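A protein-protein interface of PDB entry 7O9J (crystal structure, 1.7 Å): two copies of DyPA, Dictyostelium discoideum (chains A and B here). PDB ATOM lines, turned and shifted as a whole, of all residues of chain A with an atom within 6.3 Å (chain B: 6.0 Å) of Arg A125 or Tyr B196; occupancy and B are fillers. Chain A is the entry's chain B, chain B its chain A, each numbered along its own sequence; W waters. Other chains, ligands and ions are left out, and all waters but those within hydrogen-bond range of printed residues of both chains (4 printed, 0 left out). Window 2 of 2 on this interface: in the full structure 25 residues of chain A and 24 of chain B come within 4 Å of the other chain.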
ATOM      1  N   ALA A 120     -14.677   5.473 -30.404  1.00  0.00           N
ATOM      2  CA  ALA A 120     -14.354   4.453 -29.411  1.00  0.00           C
ATOM      3  C   ALA A 120     -15.538   4.205 -28.488  1.00  0.00           C
ATOM      4  O   ALA A 120     -15.852   3.054 -28.160  1.00  0.00           O
ATOM      5  CB  ALA A 120     -13.119   4.858 -28.605  1.00  0.00           C
ATOM      6  N   GLN A 121     -16.209   5.271 -28.060  1.00  0.00           N
ATOM      7  CA  GLN A 121     -17.310   5.094 -27.117  1.00  0.00           C
ATOM      8  C   GLN A 121     -18.489   4.394 -27.778  1.00  0.00           C
ATOM      9  O   GLN A 121     -19.082   3.474 -27.202  1.00  0.00           O
ATOM     10  CB  GLN A 121     -17.747   6.443 -26.546  1.00  0.00           C
ATOM     11  CG  GLN A 121     -18.896   6.300 -25.537  1.00  0.00           C
ATOM     12  CD  GLN A 121     -19.433   7.633 -25.054  1.00  0.00           C
ATOM     13  OE1 GLN A 121     -19.399   8.629 -25.773  1.00  0.00           O
ATOM     14  NE2 GLN A 121     -19.972   7.645 -23.843  1.00  0.00           N
ATOM     15  N   ASP A 122     -18.858   4.833 -28.988  1.00  0.00           N
ATOM     16  CA  ASP A 122     -19.965   4.202 -29.697  1.00  0.00           C
ATOM     17  C   ASP A 122     -19.685   2.726 -29.939  1.00  0.00           C
ATOM     18  O   ASP A 122     -20.588   1.882 -29.827  1.00  0.00           O
ATOM     19  CB  ASP A 122     -20.207   4.906 -31.031  1.00  0.00           C
ATOM     20  CG  ASP A 122     -20.818   6.290 -30.872  1.00  0.00           C
ATOM     21  OD1 ASP A 122     -21.181   6.686 -29.740  1.00  0.00           O
ATOM     22  OD2 ASP A 122     -20.935   6.989 -31.895  1.00  0.00           O
ATOM     23  N   THR A 123     -18.433   2.403 -30.287  1.00  0.00           N
ATOM     24  CA  THR A 123     -18.065   1.021 -30.575  1.00  0.00           C
ATOM     25  C   THR A 123     -18.173   0.164 -29.320  1.00  0.00           C
ATOM     26  O   THR A 123     -18.733  -0.939 -29.360  1.00  0.00           O
ATOM     27  CB  THR A 123     -16.651   0.975 -31.161  1.00  0.00           C
ATOM     28  OG1 THR A 123     -16.626   1.723 -32.392  1.00  0.00           O
ATOM     29  CG2 THR A 123     -16.239  -0.464 -31.455  1.00  0.00           C
ATOM     30  N   MET A 124     -17.692   0.678 -28.188  1.00  0.00           N
ATOM     31  CA  MET A 124     -17.791  -0.087 -26.952  1.00  0.00           C
ATOM     32  C   MET A 124     -19.242  -0.238 -26.508  1.00  0.00           C
ATOM     33  O   MET A 124     -19.605  -1.271 -25.937  1.00  0.00           O
ATOM     34  CB  MET A 124     -16.939   0.557 -25.859  1.00  0.00           C
ATOM     35  CG  MET A 124     -15.437   0.343 -26.012  1.00  0.00           C
ATOM     36  SD  MET A 124     -14.977  -1.381 -26.318  1.00  0.00           S
ATOM     37  CE  MET A 124     -15.846  -2.223 -24.990  1.00  0.00           C
ATOM     38  N   ARG A 125     -20.093   0.759 -26.781  1.00  0.00           N
ATOM     39  CA  ARG A 125     -21.508   0.615 -26.446  1.00  0.00           C
ATOM     40  C   ARG A 125     -22.199  -0.408 -27.344  1.00  0.00           C
ATOM     41  O   ARG A 125     -23.114  -1.108 -26.887  1.00  0.00           O
ATOM     42  CB  ARG A 125     -22.210   1.974 -26.512  1.00  0.00           C
ATOM     43  CG  ARG A 125     -21.937   2.828 -25.262  1.00  0.00           C
ATOM     44  CD  ARG A 125     -22.698   4.154 -25.252  1.00  0.00           C
ATOM     45  NE  ARG A 125     -24.116   3.984 -24.942  1.00  0.00           N
ATOM     46  CZ  ARG A 125     -25.033   4.937 -25.102  1.00  0.00           C
ATOM     47  NH1 ARG A 125     -24.678   6.129 -25.568  1.00  0.00           N
ATOM     48  NH2 ARG A 125     -26.306   4.702 -24.798  1.00  0.00           N
ATOM     49  N   ASN A 126     -21.783  -0.522 -28.613  1.00  0.00           N
ATOM     50  CA  ASN A 126     -22.365  -1.532 -29.501  1.00  0.00           C
ATOM     51  C   ASN A 126     -21.988  -2.941 -29.062  1.00  0.00           C
ATOM     52  O   ASN A 126     -22.856  -3.809 -28.930  1.00  0.00           O
ATOM     53  CB  ASN A 126     -21.914  -1.317 -30.951  1.00  0.00           C
ATOM     54  CG  ASN A 126     -22.546  -0.101 -31.592  1.00  0.00           C
ATOM     55  OD1 ASN A 126     -23.580   0.386 -31.140  1.00  0.00           O
ATOM     56  ND2 ASN A 126     -21.917   0.402 -32.651  1.00  0.00           N
ATOM     57  N   PHE A 127     -20.688  -3.195 -28.862  1.00  0.00           N
ATOM     58  CA  PHE A 127     -20.253  -4.524 -28.441  1.00  0.00           C
ATOM     59  C   PHE A 127     -20.759  -4.834 -27.036  1.00  0.00           C
ATOM     60  O   PHE A 127     -21.378  -5.879 -26.801  1.00  0.00           O
ATOM     61  CB  PHE A 127     -18.728  -4.631 -28.493  1.00  0.00           C
ATOM     62  CG  PHE A 127     -18.168  -4.803 -29.889  1.00  0.00           C
ATOM     63  CD1 PHE A 127     -18.209  -6.038 -30.526  1.00  0.00           C
ATOM     64  CD2 PHE A 127     -17.575  -3.735 -30.548  1.00  0.00           C
ATOM     65  CE1 PHE A 127     -17.682  -6.197 -31.803  1.00  0.00           C
ATOM     66  CE2 PHE A 127     -17.042  -3.883 -31.823  1.00  0.00           C
ATOM     67  CZ  PHE A 127     -17.095  -5.112 -32.455  1.00  0.00           C
ATOM     68  N   GLY A 128     -20.510  -3.936 -26.095  1.00  0.00           N
ATOM     69  CA  GLY A 128     -21.006  -4.093 -24.746  1.00  0.00           C
ATOM     70  C   GLY A 128     -20.159  -5.037 -23.908  1.00  0.00           C
ATOM     71  O   GLY A 128     -19.331  -5.802 -24.406  1.00  0.00           O
ATOM     72  N   ARG B 143     -16.245  16.971 -26.088  1.00  0.00           N
ATOM     73  CA  ARG B 143     -16.830  15.933 -26.927  1.00  0.00           C
ATOM     74  C   ARG B 143     -17.590  16.554 -28.097  1.00  0.00           C
ATOM     75  O   ARG B 143     -17.824  17.765 -28.156  1.00  0.00           O
ATOM     76  CB  ARG B 143     -17.750  15.032 -26.085  1.00  0.00           C
ATOM     77  CG  ARG B 143     -16.973  14.076 -25.200  1.00  0.00           C
ATOM     78  CD  ARG B 143     -17.918  13.304 -24.281  1.00  0.00           C
ATOM     79  NE  ARG B 143     -18.726  12.274 -24.955  1.00  0.00           N
ATOM     80  CZ  ARG B 143     -20.065  12.258 -24.967  1.00  0.00           C
ATOM     81  NH1 ARG B 143     -20.745  13.254 -24.416  1.00  0.00           N
ATOM     82  NH2 ARG B 143     -20.731  11.258 -25.535  1.00  0.00           N
ATOM     83  N   LEU B 149     -21.263  13.869 -20.850  1.00  0.00           N
ATOM     84  CA  LEU B 149     -21.490  12.433 -21.042  1.00  0.00           C
ATOM     85  C   LEU B 149     -22.941  11.991 -20.790  1.00  0.00           C
ATOM     86  O   LEU B 149     -23.301  10.873 -21.184  1.00  0.00           O
ATOM     87  CB  LEU B 149     -20.519  11.627 -20.169  1.00  0.00           C
ATOM     88  CG  LEU B 149     -19.091  11.565 -20.738  1.00  0.00           C
ATOM     89  CD1 LEU B 149     -18.082  11.207 -19.655  1.00  0.00           C
ATOM     90  CD2 LEU B 149     -19.056  10.530 -21.874  1.00  0.00           C
ATOM     91  N   THR B 150     -23.789  12.826 -20.174  1.00  0.00           N
ATOM     92  CA  THR B 150     -25.237  12.585 -20.218  1.00  0.00           C
ATOM     93  C   THR B 150     -25.803  12.729 -21.622  1.00  0.00           C
ATOM     94  O   THR B 150     -26.983  12.409 -21.842  1.00  0.00           O
ATOM     95  CB  THR B 150     -25.985  13.567 -19.333  1.00  0.00           C
ATOM     96  OG1 THR B 150     -25.659  14.904 -19.746  1.00  0.00           O
ATOM     97  CG2 THR B 150     -25.667  13.349 -17.857  1.00  0.00           C
ATOM     98  N   ASP B 151     -24.996  13.255 -22.543  1.00  0.00           N
ATOM     99  CA  ASP B 151     -25.330  13.532 -23.935  1.00  0.00           C
ATOM    100  C   ASP B 151     -26.292  14.701 -24.083  1.00  0.00           C
ATOM    101  O   ASP B 151     -26.926  14.856 -25.129  1.00  0.00           O
ATOM    102  CB  ASP B 151     -25.813  12.261 -24.641  1.00  0.00           C
ATOM    103  CG  ASP B 151     -24.661  11.281 -24.840  1.00  0.00           C
ATOM    104  OD1 ASP B 151     -23.522  11.776 -25.050  1.00  0.00           O
ATOM    105  OD2 ASP B 151     -24.858  10.049 -24.742  1.00  0.00           O
ATOM    106  N   ASN B 191     -22.890   7.969 -13.287  1.00  0.00           N
ATOM    107  CA  ASN B 191     -23.419   6.605 -13.287  1.00  0.00           C
ATOM    108  C   ASN B 191     -24.282   6.448 -14.534  1.00  0.00           C
ATOM    109  O   ASN B 191     -25.516   6.500 -14.479  1.00  0.00           O
ATOM    110  CB  ASN B 191     -24.225   6.342 -11.999  1.00  0.00           C
ATOM    111  CG  ASN B 191     -24.747   4.925 -11.918  1.00  0.00           C
ATOM    112  OD1 ASN B 191     -24.563   4.125 -12.835  1.00  0.00           O
ATOM    113  ND2 ASN B 191     -25.399   4.606 -10.811  1.00  0.00           N
ATOM    114  N   LEU B 192     -23.620   6.257 -15.674  1.00  0.00           N
ATOM    115  CA  LEU B 192     -24.350   6.235 -16.933  1.00  0.00           C
ATOM    116  C   LEU B 192     -25.192   4.979 -17.088  1.00  0.00           C
ATOM    117  O   LEU B 192     -26.180   4.999 -17.832  1.00  0.00           O
ATOM    118  CB  LEU B 192     -23.383   6.376 -18.104  1.00  0.00           C
ATOM    119  CG  LEU B 192     -22.641   7.714 -18.133  1.00  0.00           C
ATOM    120  CD1 LEU B 192     -21.678   7.754 -19.294  1.00  0.00           C
ATOM    121  CD2 LEU B 192     -23.651   8.852 -18.227  1.00  0.00           C
ATOM    122  N   LYS B 193     -24.846   3.899 -16.386  1.00  0.00           N
ATOM    123  CA  LYS B 193     -25.696   2.713 -16.418  1.00  0.00           C
ATOM    124  C   LYS B 193     -27.096   3.022 -15.910  1.00  0.00           C
ATOM    125  O   LYS B 193     -28.078   2.452 -16.403  1.00  0.00           O
ATOM    126  CB  LYS B 193     -25.071   1.589 -15.592  1.00  0.00           C
ATOM    127  CG  LYS B 193     -25.719   0.236 -15.839  1.00  0.00           C
ATOM    128  CD  LYS B 193     -25.084  -0.858 -14.995  1.00  0.00           C
ATOM    129  CE  LYS B 193     -25.054  -0.477 -13.529  1.00  0.00           C
ATOM    130  NZ  LYS B 193     -24.369  -1.519 -12.713  1.00  0.00           N
ATOM    131  N   LYS B 194     -27.208   3.924 -14.934  1.00  0.00           N
ATOM    132  CA  LYS B 194     -28.501   4.331 -14.400  1.00  0.00           C
ATOM    133  C   LYS B 194     -29.191   5.369 -15.284  1.00  0.00           C
ATOM    134  O   LYS B 194     -30.425   5.428 -15.320  1.00  0.00           O
ATOM    135  CB  LYS B 194     -28.297   4.878 -12.985  1.00  0.00           C
ATOM    136  CG  LYS B 194     -29.561   5.301 -12.262  1.00  0.00           C
ATOM    137  CD  LYS B 194     -29.251   5.682 -10.813  1.00  0.00           C
ATOM    138  CE  LYS B 194     -30.495   6.182 -10.101  1.00  0.00           C
ATOM    139  NZ  LYS B 194     -30.181   6.656  -8.725  1.00  0.00           N
ATOM    140  N   TRP B 195     -28.416   6.189 -15.994  1.00  0.00           N
ATOM    141  CA  TRP B 195     -28.956   7.286 -16.794  1.00  0.00           C
ATOM    142  C   TRP B 195     -29.475   6.818 -18.149  1.00  0.00           C
ATOM    143  O   TRP B 195     -30.589   7.178 -18.554  1.00  0.00           O
ATOM    144  CB  TRP B 195     -27.856   8.329 -16.982  1.00  0.00           C
ATOM    145  CG  TRP B 195     -28.174   9.472 -17.885  1.00  0.00           C
ATOM    146  CD1 TRP B 195     -27.632   9.719 -19.114  1.00  0.00           C
ATOM    147  CD2 TRP B 195     -29.053  10.563 -17.605  1.00  0.00           C
ATOM    148  NE1 TRP B 195     -28.136  10.887 -19.630  1.00  0.00           N
ATOM    149  CE2 TRP B 195     -29.013  11.427 -18.723  1.00  0.00           C
ATOM    150  CE3 TRP B 195     -29.884  10.889 -16.527  1.00  0.00           C
ATOM    151  CZ2 TRP B 195     -29.752  12.612 -18.780  1.00  0.00           C
ATOM    152  CZ3 TRP B 195     -30.632  12.064 -16.589  1.00  0.00           C
ATOM    153  CH2 TRP B 195     -30.558  12.909 -17.710  1.00  0.00           C
ATOM    154  N   TYR B 196     -28.667   6.044 -18.872  1.00  0.00           N
ATOM    155  CA  TYR B 196     -29.010   5.629 -20.231  1.00  0.00           C
ATOM    156  C   TYR B 196     -30.400   5.013 -20.374  1.00  0.00           C
ATOM    157  O   TYR B 196     -31.071   5.305 -21.380  1.00  0.00           O
ATOM    158  CB  TYR B 196     -27.956   4.629 -20.732  1.00  0.00           C
ATOM    159  CG  TYR B 196     -26.621   5.209 -21.144  1.00  0.00           C
ATOM    160  CD1 TYR B 196     -26.496   6.534 -21.565  1.00  0.00           C
ATOM    161  CD2 TYR B 196     -25.486   4.413 -21.144  1.00  0.00           C
ATOM    162  CE1 TYR B 196     -25.260   7.046 -21.963  1.00  0.00           C
ATOM    163  CE2 TYR B 196     -24.258   4.910 -21.544  1.00  0.00           C
ATOM    164  CZ  TYR B 196     -24.148   6.221 -21.953  1.00  0.00           C
ATOM    165  OH  TYR B 196     -22.908   6.689 -22.359  1.00  0.00           O
ATOM    166  N   PRO B 197     -30.890   4.176 -19.450  1.00  0.00           N
ATOM    167  CA  PRO B 197     -32.224   3.579 -19.627  1.00  0.00           C
ATOM    168  C   PRO B 197     -33.389   4.518 -19.368  1.00  0.00           C
ATOM    169  O   PRO B 197     -34.534   4.128 -19.637  1.00  0.00           O
ATOM    170  CB  PRO B 197     -32.240   2.434 -18.598  1.00  0.00           C
ATOM    171  CG  PRO B 197     -30.835   2.292 -18.132  1.00  0.00           C
ATOM    172  CD  PRO B 197     -30.191   3.602 -18.288  1.00  0.00           C
ATOM    173  N   GLU B 198     -33.157   5.706 -18.821  1.00  0.00           N
ATOM    174  CA  GLU B 198     -34.271   6.596 -18.531  1.00  0.00           C
ATOM    175  C   GLU B 198     -34.911   7.078 -19.832  1.00  0.00           C
ATOM    176  O   GLU B 198     -34.203   7.378 -20.802  1.00  0.00           O
ATOM    177  CB  GLU B 198     -33.813   7.798 -17.705  1.00  0.00           C
ATOM    178  CG  GLU B 198     -33.329   7.448 -16.303  1.00  0.00           C
ATOM    179  CD  GLU B 198     -34.465   7.188 -15.320  1.00  0.00           C
ATOM    180  OE1 GLU B 198     -34.230   7.334 -14.103  1.00  0.00           O
ATOM    181  OE2 GLU B 198     -35.591   6.841 -15.754  1.00  0.00           O
ATOM    182  N   PRO B 199     -36.240   7.158 -19.883  1.00  0.00           N
ATOM    183  CA  PRO B 199     -36.899   7.723 -21.065  1.00  0.00           C
ATOM    184  C   PRO B 199     -36.479   9.167 -21.286  1.00  0.00           C
ATOM    185  O   PRO B 199     -36.087   9.875 -20.351  1.00  0.00           O
ATOM    186  CB  PRO B 199     -38.392   7.631 -20.721  1.00  0.00           C
ATOM    187  CG  PRO B 199     -38.483   6.648 -19.607  1.00  0.00           C
ATOM    188  CD  PRO B 199     -37.202   6.730 -18.853  1.00  0.00           C
ATOM    189  N   GLN B 203     -35.197  12.221 -18.722  1.00  0.00           N
ATOM    190  CA  GLN B 203     -33.907  12.904 -18.850  1.00  0.00           C
ATOM    191  C   GLN B 203     -34.097  14.404 -19.016  1.00  0.00           C
ATOM    192  O   GLN B 203     -33.359  15.201 -18.416  1.00  0.00           O
ATOM    193  CB  GLN B 203     -33.115  12.335 -20.032  1.00  0.00           C
ATOM    194  CG  GLN B 203     -32.687  10.887 -19.829  1.00  0.00           C
ATOM    195  CD  GLN B 203     -31.719  10.420 -20.905  1.00  0.00           C
ATOM    196  OE1 GLN B 203     -31.456  11.142 -21.865  1.00  0.00           O
ATOM    197  NE2 GLN B 203     -31.182   9.212 -20.746  1.00  0.00           N
ATOM    198  N   ILE B 252     -13.807   5.245 -21.161  1.00  0.00           N
ATOM    199  CA  ILE B 252     -15.039   4.620 -21.658  1.00  0.00           C
ATOM    200  C   ILE B 252     -15.383   3.379 -20.845  1.00  0.00           C
ATOM    201  O   ILE B 252     -16.549   3.158 -20.474  1.00  0.00           O
ATOM    202  CB  ILE B 252     -14.891   4.285 -23.155  1.00  0.00           C
ATOM    203  CG1 ILE B 252     -14.798   5.573 -23.966  1.00  0.00           C
ATOM    204  CG2 ILE B 252     -16.077   3.424 -23.661  1.00  0.00           C
ATOM    205  CD1 ILE B 252     -14.092   5.403 -25.286  1.00  0.00           C
ATOM    206  N   LYS B 256     -15.636   7.785 -15.382  1.00  0.00           N
ATOM    207  CA  LYS B 256     -15.735   8.952 -16.251  1.00  0.00           C
ATOM    208  C   LYS B 256     -16.798   9.893 -15.708  1.00  0.00           C
ATOM    209  O   LYS B 256     -17.629   9.511 -14.884  1.00  0.00           O
ATOM    210  CB  LYS B 256     -16.085   8.543 -17.689  1.00  0.00           C
ATOM    211  CG  LYS B 256     -17.318   7.639 -17.795  1.00  0.00           C
ATOM    212  CD  LYS B 256     -17.499   7.160 -19.229  1.00  0.00           C
ATOM    213  CE  LYS B 256     -18.351   5.896 -19.309  1.00  0.00           C
ATOM    214  NZ  LYS B 256     -17.813   4.779 -18.478  1.00  0.00           N
HETATM  215  O   HOH W   1     -20.281   5.229 -22.290  1.00  0.00           O
HETATM  216  O   HOH W   2     -23.169   8.589 -26.370  1.00  0.00           O
HETATM  217  O   HOH W   3     -18.632  11.088 -27.799  1.00  0.00           O
HETATM  218  O   HOH W   4     -22.502   9.148 -23.086  1.00  0.00           O
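NH2 of Arg B143 is in hydrogen-bond range of OE1 of Gln A121, 3.0 Å away.
The side-chain hydroxyl of Tyr B196 sits at hydrogen-bond distance from the side-chain amide nitrogen of Gln A121 (3.4 Å).
NH2 of Arg B143 lies within salt-bridge range of OD1 of Asp B151.
O of Ile B252 lies within hydrogen-bond range of NZ of Lys B256, 2.9 Å away.
CB of Ala A120 touches CD1 of Ile B252, 3.5 Å away.
Gln A121 touches Leu B149 (NE2 to CD2, 3.6 Å).
CD1 of Ile B252 touches N of Gln A121 (3.5 Å).
Met A124 touches Ile B252 (CB to CG2, 3.7 Å).
Tyr B196 touches Arg A125.
Of the printed residues of chain B, Gln A121 touches Arg B143 (3.0 Å), Leu B149 (3.6 Å), Tyr B196 (3.4 Å) and Ile B252 (3.5 Å).
Printed residues of chain B within 4 Å of Arg A125: Tyr B196 (3.5 Å).
Printed residues of chain A within 4 Å of Leu B149: Gln A121.
Leu B192 touches none of the printed residues of chain A.
Tyr B196 touches just these residues of chain A: Gln A121 and Arg A125.
Of the printed residues of chain A, Ile B252 touches Ala A120, Gln A121 and Met A124.
The nearest printed residue of chain A that does not touch Ile B252 is Arg A125 (5.7 Å).
Hydrophobic or aromatic side chains of chain A within 4 Å of the printed part of chain B: Ala A120 and Met A124.
No position is printed for both chains.
Of the 7 pairs that touch across the chains among the printed residues, none has its exchanged pair printed and touching as well.
Water W4 lies within hydrogen-bond range of OH of Tyr B196 (2.6 Å), O of Leu B149 (2.7 Å), OD2 of Asp B151 (3.0 Å) and NE2 of Gln A121 (3.0 Å).
Water W2 bridges the side-chain carboxylate of Asp B151 (2.8 Å) and the guanidinium group of Arg A125 (3.0 Å).
Water W1 bridges the side-chain amide nitrogen (NE2) of Gln A121 (2.9 Å) and the side-chain hydroxyl (OH) of Tyr B196 (3.0 Å).
Water W3 bridges the guanidinium group of Arg B143 and the side-chain amide oxygen of Gln A121.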
